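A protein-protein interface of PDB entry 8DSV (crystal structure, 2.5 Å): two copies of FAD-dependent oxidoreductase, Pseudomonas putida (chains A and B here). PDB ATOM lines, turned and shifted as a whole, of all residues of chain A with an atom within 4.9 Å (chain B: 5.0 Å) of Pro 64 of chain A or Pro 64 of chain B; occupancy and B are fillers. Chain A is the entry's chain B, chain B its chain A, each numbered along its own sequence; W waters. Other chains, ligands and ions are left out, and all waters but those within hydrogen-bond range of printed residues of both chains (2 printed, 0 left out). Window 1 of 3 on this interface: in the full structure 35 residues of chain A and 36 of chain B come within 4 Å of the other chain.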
ATOM      1  N   TRP A  61      21.150  20.762 -17.731  1.00  0.00           N
ATOM      2  CA  TRP A  61      20.934  21.946 -18.560  1.00  0.00           C
ATOM      3  C   TRP A  61      22.135  22.889 -18.577  1.00  0.00           C
ATOM      4  O   TRP A  61      22.218  23.747 -19.462  1.00  0.00           O
ATOM      5  CB  TRP A  61      19.687  22.712 -18.102  1.00  0.00           C
ATOM      6  CG  TRP A  61      19.588  22.908 -16.621  1.00  0.00           C
ATOM      7  CD1 TRP A  61      20.068  23.963 -15.896  1.00  0.00           C
ATOM      8  CD2 TRP A  61      18.973  22.022 -15.682  1.00  0.00           C
ATOM      9  NE1 TRP A  61      19.792  23.784 -14.563  1.00  0.00           N
ATOM     10  CE2 TRP A  61      19.119  22.600 -14.405  1.00  0.00           C
ATOM     11  CE3 TRP A  61      18.319  20.793 -15.795  1.00  0.00           C
ATOM     12  CZ2 TRP A  61      18.630  21.993 -13.253  1.00  0.00           C
ATOM     13  CZ3 TRP A  61      17.834  20.189 -14.648  1.00  0.00           C
ATOM     14  CH2 TRP A  61      17.992  20.790 -13.392  1.00  0.00           C
ATOM     15  N   LEU A  62      23.051  22.776 -17.617  1.00  0.00           N
ATOM     16  CA  LEU A  62      24.322  23.486 -17.692  1.00  0.00           C
ATOM     17  C   LEU A  62      25.285  22.843 -18.683  1.00  0.00           C
ATOM     18  O   LEU A  62      26.419  23.319 -18.830  1.00  0.00           O
ATOM     19  CB  LEU A  62      24.970  23.562 -16.307  1.00  0.00           C
ATOM     20  CG  LEU A  62      24.104  24.267 -15.254  1.00  0.00           C
ATOM     21  CD1 LEU A  62      24.748  24.175 -13.890  1.00  0.00           C
ATOM     22  CD2 LEU A  62      23.843  25.727 -15.634  1.00  0.00           C
ATOM     23  N   GLN A  63      24.871  21.757 -19.340  1.00  0.00           N
ATOM     24  CA  GLN A  63      25.647  21.122 -20.394  1.00  0.00           C
ATOM     25  C   GLN A  63      25.040  21.539 -21.727  1.00  0.00           C
ATOM     26  O   GLN A  63      23.982  21.015 -22.111  1.00  0.00           O
ATOM     27  CB  GLN A  63      25.641  19.599 -20.238  1.00  0.00           C
ATOM     28  CG  GLN A  63      26.405  19.141 -18.996  1.00  0.00           C
ATOM     29  CD  GLN A  63      26.231  17.670 -18.680  1.00  0.00           C
ATOM     30  OE1 GLN A  63      25.248  17.044 -19.071  1.00  0.00           O
ATOM     31  NE2 GLN A  63      27.192  17.110 -17.956  1.00  0.00           N
ATOM     32  N   PRO A  64      25.655  22.471 -22.466  1.00  0.00           N
ATOM     33  CA  PRO A  64      24.907  23.164 -23.535  1.00  0.00           C
ATOM     34  C   PRO A  64      24.462  22.272 -24.683  1.00  0.00           C
ATOM     35  O   PRO A  64      23.295  22.319 -25.098  1.00  0.00           O
ATOM     36  CB  PRO A  64      25.904  24.228 -24.026  1.00  0.00           C
ATOM     37  CG  PRO A  64      27.016  24.261 -23.067  1.00  0.00           C
ATOM     38  CD  PRO A  64      27.011  23.014 -22.274  1.00  0.00           C
ATOM     39  N   HIS A  65      25.365  21.451 -25.212  1.00  0.00           N
ATOM     40  CA  HIS A  65      25.102  20.796 -26.488  1.00  0.00           C
ATOM     41  C   HIS A  65      24.023  19.725 -26.350  1.00  0.00           C
ATOM     42  O   HIS A  65      23.057  19.687 -27.132  1.00  0.00           O
ATOM     43  CB  HIS A  65      26.409  20.216 -27.032  1.00  0.00           C
ATOM     44  CG  HIS A  65      27.579  21.142 -26.875  1.00  0.00           C
ATOM     45  ND1 HIS A  65      28.386  21.137 -25.758  1.00  0.00           N
ATOM     46  CD2 HIS A  65      28.063  22.117 -27.681  1.00  0.00           C
ATOM     47  CE1 HIS A  65      29.323  22.060 -25.886  1.00  0.00           C
ATOM     48  NE2 HIS A  65      29.148  22.672 -27.044  1.00  0.00           N
ATOM     49  N   VAL A  66      24.148  18.860 -25.343  1.00  0.00           N
ATOM     50  CA  VAL A  66      23.150  17.808 -25.189  1.00  0.00           C
ATOM     51  C   VAL A  66      21.809  18.386 -24.748  1.00  0.00           C
ATOM     52  O   VAL A  66      20.753  17.883 -25.147  1.00  0.00           O
ATOM     53  CB  VAL A  66      23.647  16.729 -24.212  1.00  0.00           C
ATOM     54  CG1 VAL A  66      23.635  17.252 -22.781  1.00  0.00           C
ATOM     55  CG2 VAL A  66      22.790  15.476 -24.338  1.00  0.00           C
ATOM     56  N   TRP A  67      21.813  19.452 -23.942  1.00  0.00           N
ATOM     57  CA  TRP A  67      20.546  20.064 -23.554  1.00  0.00           C
ATOM     58  C   TRP A  67      19.836  20.673 -24.758  1.00  0.00           C
ATOM     59  O   TRP A  67      18.608  20.555 -24.890  1.00  0.00           O
ATOM     60  CB  TRP A  67      20.765  21.128 -22.478  1.00  0.00           C
ATOM     61  CG  TRP A  67      19.476  21.584 -21.888  1.00  0.00           C
ATOM     62  CD1 TRP A  67      18.809  22.739 -22.166  1.00  0.00           C
ATOM     63  CD2 TRP A  67      18.672  20.875 -20.938  1.00  0.00           C
ATOM     64  NE1 TRP A  67      17.646  22.800 -21.441  1.00  0.00           N
ATOM     65  CE2 TRP A  67      17.538  21.668 -20.679  1.00  0.00           C
ATOM     66  CE3 TRP A  67      18.805  19.649 -20.279  1.00  0.00           C
ATOM     67  CZ2 TRP A  67      16.544  21.278 -19.788  1.00  0.00           C
ATOM     68  CZ3 TRP A  67      17.818  19.264 -19.394  1.00  0.00           C
ATOM     69  CH2 TRP A  67      16.701  20.076 -19.156  1.00  0.00           C
ATOM     70  N   ALA A  68      20.586  21.330 -25.647  1.00  0.00           N
ATOM     71  CA  ALA A  68      19.976  21.865 -26.858  1.00  0.00           C
ATOM     72  C   ALA A  68      19.407  20.746 -27.721  1.00  0.00           C
ATOM     73  O   ALA A  68      18.329  20.893 -28.308  1.00  0.00           O
ATOM     74  CB  ALA A  68      20.994  22.686 -27.643  1.00  0.00           C
ATOM     75  N   HIS A 128      35.988  26.399 -21.873  1.00  0.00           N
ATOM     76  CA  HIS A 128      35.966  25.882 -23.235  1.00  0.00           C
ATOM     77  C   HIS A 128      37.160  26.347 -24.063  1.00  0.00           C
ATOM     78  O   HIS A 128      37.218  26.052 -25.262  1.00  0.00           O
ATOM     79  CB  HIS A 128      34.660  26.287 -23.921  1.00  0.00           C
ATOM     80  CG  HIS A 128      33.438  25.711 -23.270  1.00  0.00           C
ATOM     81  ND1 HIS A 128      32.849  24.541 -23.697  1.00  0.00           N
ATOM     82  CD2 HIS A 128      32.704  26.139 -22.215  1.00  0.00           C
ATOM     83  CE1 HIS A 128      31.799  24.277 -22.939  1.00  0.00           C
ATOM     84  NE2 HIS A 128      31.690  25.231 -22.031  1.00  0.00           N
ATOM     85  N   TRP A 409      32.800  19.465 -21.648  1.00  0.00           N
ATOM     86  CA  TRP A 409      32.398  18.348 -20.791  1.00  0.00           C
ATOM     87  C   TRP A 409      32.920  17.054 -21.411  1.00  0.00           C
ATOM     88  O   TRP A 409      32.184  16.266 -22.008  1.00  0.00           O
ATOM     89  CB  TRP A 409      30.881  18.320 -20.635  1.00  0.00           C
ATOM     90  CG  TRP A 409      30.292  19.474 -19.838  1.00  0.00           C
ATOM     91  CD1 TRP A 409      29.828  20.661 -20.333  1.00  0.00           C
ATOM     92  CD2 TRP A 409      30.089  19.531 -18.417  1.00  0.00           C
ATOM     93  NE1 TRP A 409      29.359  21.451 -19.315  1.00  0.00           N
ATOM     94  CE2 TRP A 409      29.504  20.781 -18.129  1.00  0.00           C
ATOM     95  CE3 TRP A 409      30.347  18.649 -17.363  1.00  0.00           C
ATOM     96  CZ2 TRP A 409      29.181  21.174 -16.830  1.00  0.00           C
ATOM     97  CZ3 TRP A 409      30.023  19.040 -16.072  1.00  0.00           C
ATOM     98  CH2 TRP A 409      29.448  20.289 -15.818  1.00  0.00           C
ATOM     99  N   ASP A 414      27.813  15.226 -23.246  1.00  0.00           N
ATOM    100  CA  ASP A 414      27.821  16.559 -23.831  1.00  0.00           C
ATOM    101  C   ASP A 414      29.079  16.794 -24.653  1.00  0.00           C
ATOM    102  O   ASP A 414      29.016  17.395 -25.731  1.00  0.00           O
ATOM    103  CB  ASP A 414      27.700  17.613 -22.733  1.00  0.00           C
ATOM    104  CG  ASP A 414      27.618  19.013 -23.292  1.00  0.00           C
ATOM    105  OD1 ASP A 414      26.508  19.429 -23.684  1.00  0.00           O
ATOM    106  OD2 ASP A 414      28.667  19.689 -23.360  1.00  0.00           O
ATOM    107  N   TRP B  61      28.522  30.655 -21.898  1.00  0.00           N
ATOM    108  CA  TRP B  61      28.489  29.212 -22.121  1.00  0.00           C
ATOM    109  C   TRP B  61      27.532  28.489 -21.185  1.00  0.00           C
ATOM    110  O   TRP B  61      27.152  27.352 -21.475  1.00  0.00           O
ATOM    111  CB  TRP B  61      29.890  28.588 -21.989  1.00  0.00           C
ATOM    112  CG  TRP B  61      30.729  29.076 -20.851  1.00  0.00           C
ATOM    113  CD1 TRP B  61      30.844  28.511 -19.618  1.00  0.00           C
ATOM    114  CD2 TRP B  61      31.608  30.208 -20.859  1.00  0.00           C
ATOM    115  NE1 TRP B  61      31.727  29.232 -18.847  1.00  0.00           N
ATOM    116  CE2 TRP B  61      32.209  30.279 -19.587  1.00  0.00           C
ATOM    117  CE3 TRP B  61      31.936  31.174 -21.815  1.00  0.00           C
ATOM    118  CZ2 TRP B  61      33.118  31.279 -19.247  1.00  0.00           C
ATOM    119  CZ3 TRP B  61      32.835  32.166 -21.476  1.00  0.00           C
ATOM    120  CH2 TRP B  61      33.415  32.212 -20.202  1.00  0.00           C
ATOM    121  N   LEU B  62      27.133  29.113 -20.076  1.00  0.00           N
ATOM    122  CA  LEU B  62      26.072  28.550 -19.252  1.00  0.00           C
ATOM    123  C   LEU B  62      24.696  28.725 -19.877  1.00  0.00           C
ATOM    124  O   LEU B  62      23.701  28.273 -19.296  1.00  0.00           O
ATOM    125  CB  LEU B  62      26.075  29.193 -17.865  1.00  0.00           C
ATOM    126  CG  LEU B  62      27.344  29.047 -17.024  1.00  0.00           C
ATOM    127  CD1 LEU B  62      27.243  29.931 -15.786  1.00  0.00           C
ATOM    128  CD2 LEU B  62      27.584  27.591 -16.638  1.00  0.00           C
ATOM    129  N   GLN B  63      24.619  29.362 -21.042  1.00  0.00           N
ATOM    130  CA  GLN B  63      23.376  29.518 -21.777  1.00  0.00           C
ATOM    131  C   GLN B  63      23.356  28.477 -22.893  1.00  0.00           C
ATOM    132  O   GLN B  63      24.017  28.667 -23.924  1.00  0.00           O
ATOM    133  CB  GLN B  63      23.272  30.937 -22.339  1.00  0.00           C
ATOM    134  CG  GLN B  63      23.048  31.953 -21.235  1.00  0.00           C
ATOM    135  CD  GLN B  63      23.226  33.388 -21.681  1.00  0.00           C
ATOM    136  OE1 GLN B  63      23.853  33.665 -22.702  1.00  0.00           O
ATOM    137  NE2 GLN B  63      22.675  34.315 -20.905  1.00  0.00           N
ATOM    138  N   PRO B  64      22.618  27.375 -22.745  1.00  0.00           N
ATOM    139  CA  PRO B  64      22.887  26.181 -23.563  1.00  0.00           C
ATOM    140  C   PRO B  64      22.630  26.339 -25.058  1.00  0.00           C
ATOM    141  O   PRO B  64      23.432  25.882 -25.881  1.00  0.00           O
ATOM    142  CB  PRO B  64      21.964  25.122 -22.940  1.00  0.00           C
ATOM    143  CG  PRO B  64      20.906  25.869 -22.261  1.00  0.00           C
ATOM    144  CD  PRO B  64      21.546  27.137 -21.765  1.00  0.00           C
ATOM    145  N   HIS B  65      21.506  26.951 -25.423  1.00  0.00           N
ATOM    146  CA  HIS B  65      21.056  26.913 -26.814  1.00  0.00           C
ATOM    147  C   HIS B  65      21.943  27.775 -27.709  1.00  0.00           C
ATOM    148  O   HIS B  65      22.398  27.332 -28.776  1.00  0.00           O
ATOM    149  CB  HIS B  65      19.590  27.349 -26.881  1.00  0.00           C
ATOM    150  CG  HIS B  65      18.721  26.654 -25.878  1.00  0.00           C
ATOM    151  ND1 HIS B  65      18.428  27.194 -24.644  1.00  0.00           N
ATOM    152  CD2 HIS B  65      18.113  25.444 -25.911  1.00  0.00           C
ATOM    153  CE1 HIS B  65      17.663  26.355 -23.968  1.00  0.00           C
ATOM    154  NE2 HIS B  65      17.456  25.286 -24.715  1.00  0.00           N
ATOM    155  N   VAL B  66      22.218  29.009 -27.285  1.00  0.00           N
ATOM    156  CA  VAL B  66      23.056  29.881 -28.098  1.00  0.00           C
ATOM    157  C   VAL B  66      24.499  29.387 -28.107  1.00  0.00           C
ATOM    158  O   VAL B  66      25.198  29.518 -29.117  1.00  0.00           O
ATOM    159  CB  VAL B  66      22.946  31.340 -27.609  1.00  0.00           C
ATOM    160  CG1 VAL B  66      23.498  31.496 -26.187  1.00  0.00           C
ATOM    161  CG2 VAL B  66      23.645  32.285 -28.580  1.00  0.00           C
ATOM    162  N   TRP B  67      24.968  28.792 -27.006  1.00  0.00           N
ATOM    163  CA  TRP B  67      26.321  28.237 -27.006  1.00  0.00           C
ATOM    164  C   TRP B  67      26.432  27.064 -27.972  1.00  0.00           C
ATOM    165  O   TRP B  67      27.445  26.920 -28.670  1.00  0.00           O
ATOM    166  CB  TRP B  67      26.729  27.811 -25.594  1.00  0.00           C
ATOM    167  CG  TRP B  67      28.208  27.571 -25.479  1.00  0.00           C
ATOM    168  CD1 TRP B  67      28.835  26.365 -25.391  1.00  0.00           C
ATOM    169  CD2 TRP B  67      29.246  28.564 -25.459  1.00  0.00           C
ATOM    170  NE1 TRP B  67      30.197  26.542 -25.312  1.00  0.00           N
ATOM    171  CE2 TRP B  67      30.475  27.883 -25.354  1.00  0.00           C
ATOM    172  CE3 TRP B  67      29.254  29.961 -25.512  1.00  0.00           C
ATOM    173  CZ2 TRP B  67      31.702  28.552 -25.299  1.00  0.00           C
ATOM    174  CZ3 TRP B  67      30.473  30.624 -25.459  1.00  0.00           C
ATOM    175  CH2 TRP B  67      31.679  29.917 -25.355  1.00  0.00           C
ATOM    176  N   ALA B  68      25.405  26.211 -28.025  1.00  0.00           N
ATOM    177  CA  ALA B  68      25.411  25.117 -28.990  1.00  0.00           C
ATOM    178  C   ALA B  68      25.423  25.648 -30.417  1.00  0.00           C
ATOM    179  O   ALA B  68      26.119  25.107 -31.286  1.00  0.00           O
ATOM    180  CB  ALA B  68      24.194  24.223 -28.767  1.00  0.00           C
ATOM    181  N   HIS B 128      14.461  25.278 -15.965  1.00  0.00           N
ATOM    182  CA  HIS B 128      13.785  25.153 -17.250  1.00  0.00           C
ATOM    183  C   HIS B 128      12.417  24.488 -17.136  1.00  0.00           C
ATOM    184  O   HIS B 128      11.792  24.210 -18.163  1.00  0.00           O
ATOM    185  CB  HIS B 128      14.675  24.386 -18.234  1.00  0.00           C
ATOM    186  CG  HIS B 128      15.950  25.101 -18.564  1.00  0.00           C
ATOM    187  ND1 HIS B 128      16.102  25.866 -19.701  1.00  0.00           N
ATOM    188  CD2 HIS B 128      17.123  25.187 -17.893  1.00  0.00           C
ATOM    189  CE1 HIS B 128      17.318  26.383 -19.721  1.00  0.00           C
ATOM    190  NE2 HIS B 128      17.958  25.986 -18.635  1.00  0.00           N
ATOM    191  N   TRP B 409      16.361  31.239 -20.186  1.00  0.00           N
ATOM    192  CA  TRP B 409      16.912  32.594 -20.209  1.00  0.00           C
ATOM    193  C   TRP B 409      15.972  33.485 -21.020  1.00  0.00           C
ATOM    194  O   TRP B 409      16.220  33.822 -22.181  1.00  0.00           O
ATOM    195  CB  TRP B 409      18.317  32.583 -20.798  1.00  0.00           C
ATOM    196  CG  TRP B 409      19.342  31.899 -19.945  1.00  0.00           C
ATOM    197  CD1 TRP B 409      19.697  30.586 -19.991  1.00  0.00           C
ATOM    198  CD2 TRP B 409      20.153  32.500 -18.924  1.00  0.00           C
ATOM    199  NE1 TRP B 409      20.674  30.326 -19.061  1.00  0.00           N
ATOM    200  CE2 TRP B 409      20.973  31.486 -18.394  1.00  0.00           C
ATOM    201  CE3 TRP B 409      20.263  33.797 -18.408  1.00  0.00           C
ATOM    202  CZ2 TRP B 409      21.892  31.725 -17.373  1.00  0.00           C
ATOM    203  CZ3 TRP B 409      21.175  34.031 -17.395  1.00  0.00           C
ATOM    204  CH2 TRP B 409      21.978  32.999 -16.888  1.00  0.00           C
ATOM    205  N   ASP B 414      19.409  33.629 -25.627  1.00  0.00           N
ATOM    206  CA  ASP B 414      19.329  32.181 -25.488  1.00  0.00           C
ATOM    207  C   ASP B 414      17.884  31.701 -25.442  1.00  0.00           C
ATOM    208  O   ASP B 414      17.548  30.679 -26.050  1.00  0.00           O
ATOM    209  CB  ASP B 414      20.086  31.739 -24.237  1.00  0.00           C
ATOM    210  CG  ASP B 414      20.129  30.238 -24.086  1.00  0.00           C
ATOM    211  OD1 ASP B 414      20.993  29.604 -24.728  1.00  0.00           O
ATOM    212  OD2 ASP B 414      19.297  29.695 -23.328  1.00  0.00           O
HETATM  213  O   HOH W   1      15.606  23.947 -23.163  1.00  0.00           O
HETATM  214  O   HOH W   2      31.232  24.857 -27.527  1.00  0.00           O
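The backbone NH (N) of His 65 of chain B sits at hydrogen-bond distance from the side-chain carboxylate (OD1) of Asp 414 of chain B (2.8 Å).
Pro 64 of chain B touches Trp 61 of chain A.
CB of Trp 61 of chain A touches CD2 of His 128 of chain B, at 3.6 Å.
Trp 61 of chain B touches Pro 64 of chain A (O to CG, 3.5 Å).
Pro 64 of chain A touches Trp 67 of chain B (CG to CD1, 3.6 Å).
CD1 of Trp 67 of chain A touches CG of Pro 64 of chain B (3.8 Å).
Trp 67 of chain A touches His 65 of chain B (CD1 to NE2, 3.8 Å).
His 128 of chain B touches Trp 67 of chain A (ND1 to NE1, 3.8 Å).
Ala 68 of chain B touches Ala 68 of chain A (CB to CB, 3.7 Å).
CB of Trp 61 of chain B touches CD2 of His 128 of chain A, 3.7 Å away.
His 128 of chain A touches Trp 67 of chain B (CE1 to NE1, 3.7 Å).
Pro 64 of chain A touches just these residues of chain B: Trp 61, Pro 64 and Trp 67.
Of chain A, only Trp 61 (3.7 Å), Pro 64 (3.5 Å) and Trp 67 (3.8 Å) come within 4 Å of Pro 64 of chain B.
Of the printed residues of chain B, Trp 61 of chain A touches Pro 64 and His 128.
Of the printed residues of chain B, Trp 67 of chain A touches Pro 64 (3.8 Å), His 65 (3.8 Å) and His 128 (3.8 Å).
His 65 of chain A touches none of the printed residues of chain B.
The nearest residue of chain B that does not touch Pro 64 of chain A is Ala 68 of chain B (4.2 Å).
The nearest residue of chain A that does not touch Pro 64 of chain B is Ala 68 of chain A (4.4 Å).
The nearest printed residue of chain A that does not touch His 65 of chain B is Ala 68 of chain A (4.1 Å).
Printed residues of chain B that touch a printed residue of chain A: Trp 61, Pro 64, His 65, Trp 67, Ala 68 and His 128.
Hydrophobic or aromatic side chains of chain B within 4 Å of the printed part of chain A: Trp 61, Pro 64, His 65, Trp 67, Ala 68 and His 128.
Hydrophobic or aromatic side chains of chain A within 4 Å of the printed part of chain B: Trp 61, Pro 64, Trp 67, Ala 68 and His 128.
Among the printed residues, no Asp or Glu carboxylate lies within 4 Å of a Lys or Arg side-chain nitrogen of the other chain.
Trp 61 of chain A touches Pro 64 of chain B, and with the chains exchanged Pro 64 of chain A touches Trp 61 of chain B.
Trp 61 of chain A touches His 128 of chain B, and with the chains exchanged His 128 of chain A touches Trp 61 of chain B.
Pro 64 of chain A touches Trp 67 of chain B, and with the chains exchanged Trp 67 of chain A touches Pro 64 of chain B.
Trp 67 of chain A touches His 128 of chain B, and with the chains exchanged His 128 of chain A touches Trp 67 of chain B.
Water W1 bridges a ring nitrogen (NE2) of His 65 of chain B and the indole nitrogen of Trp 67 of chain A.
Water W2 bridges the indole nitrogen (NE1) of Trp 67 of chain B and a ring nitrogen (NE2) of His 65 of chain A.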
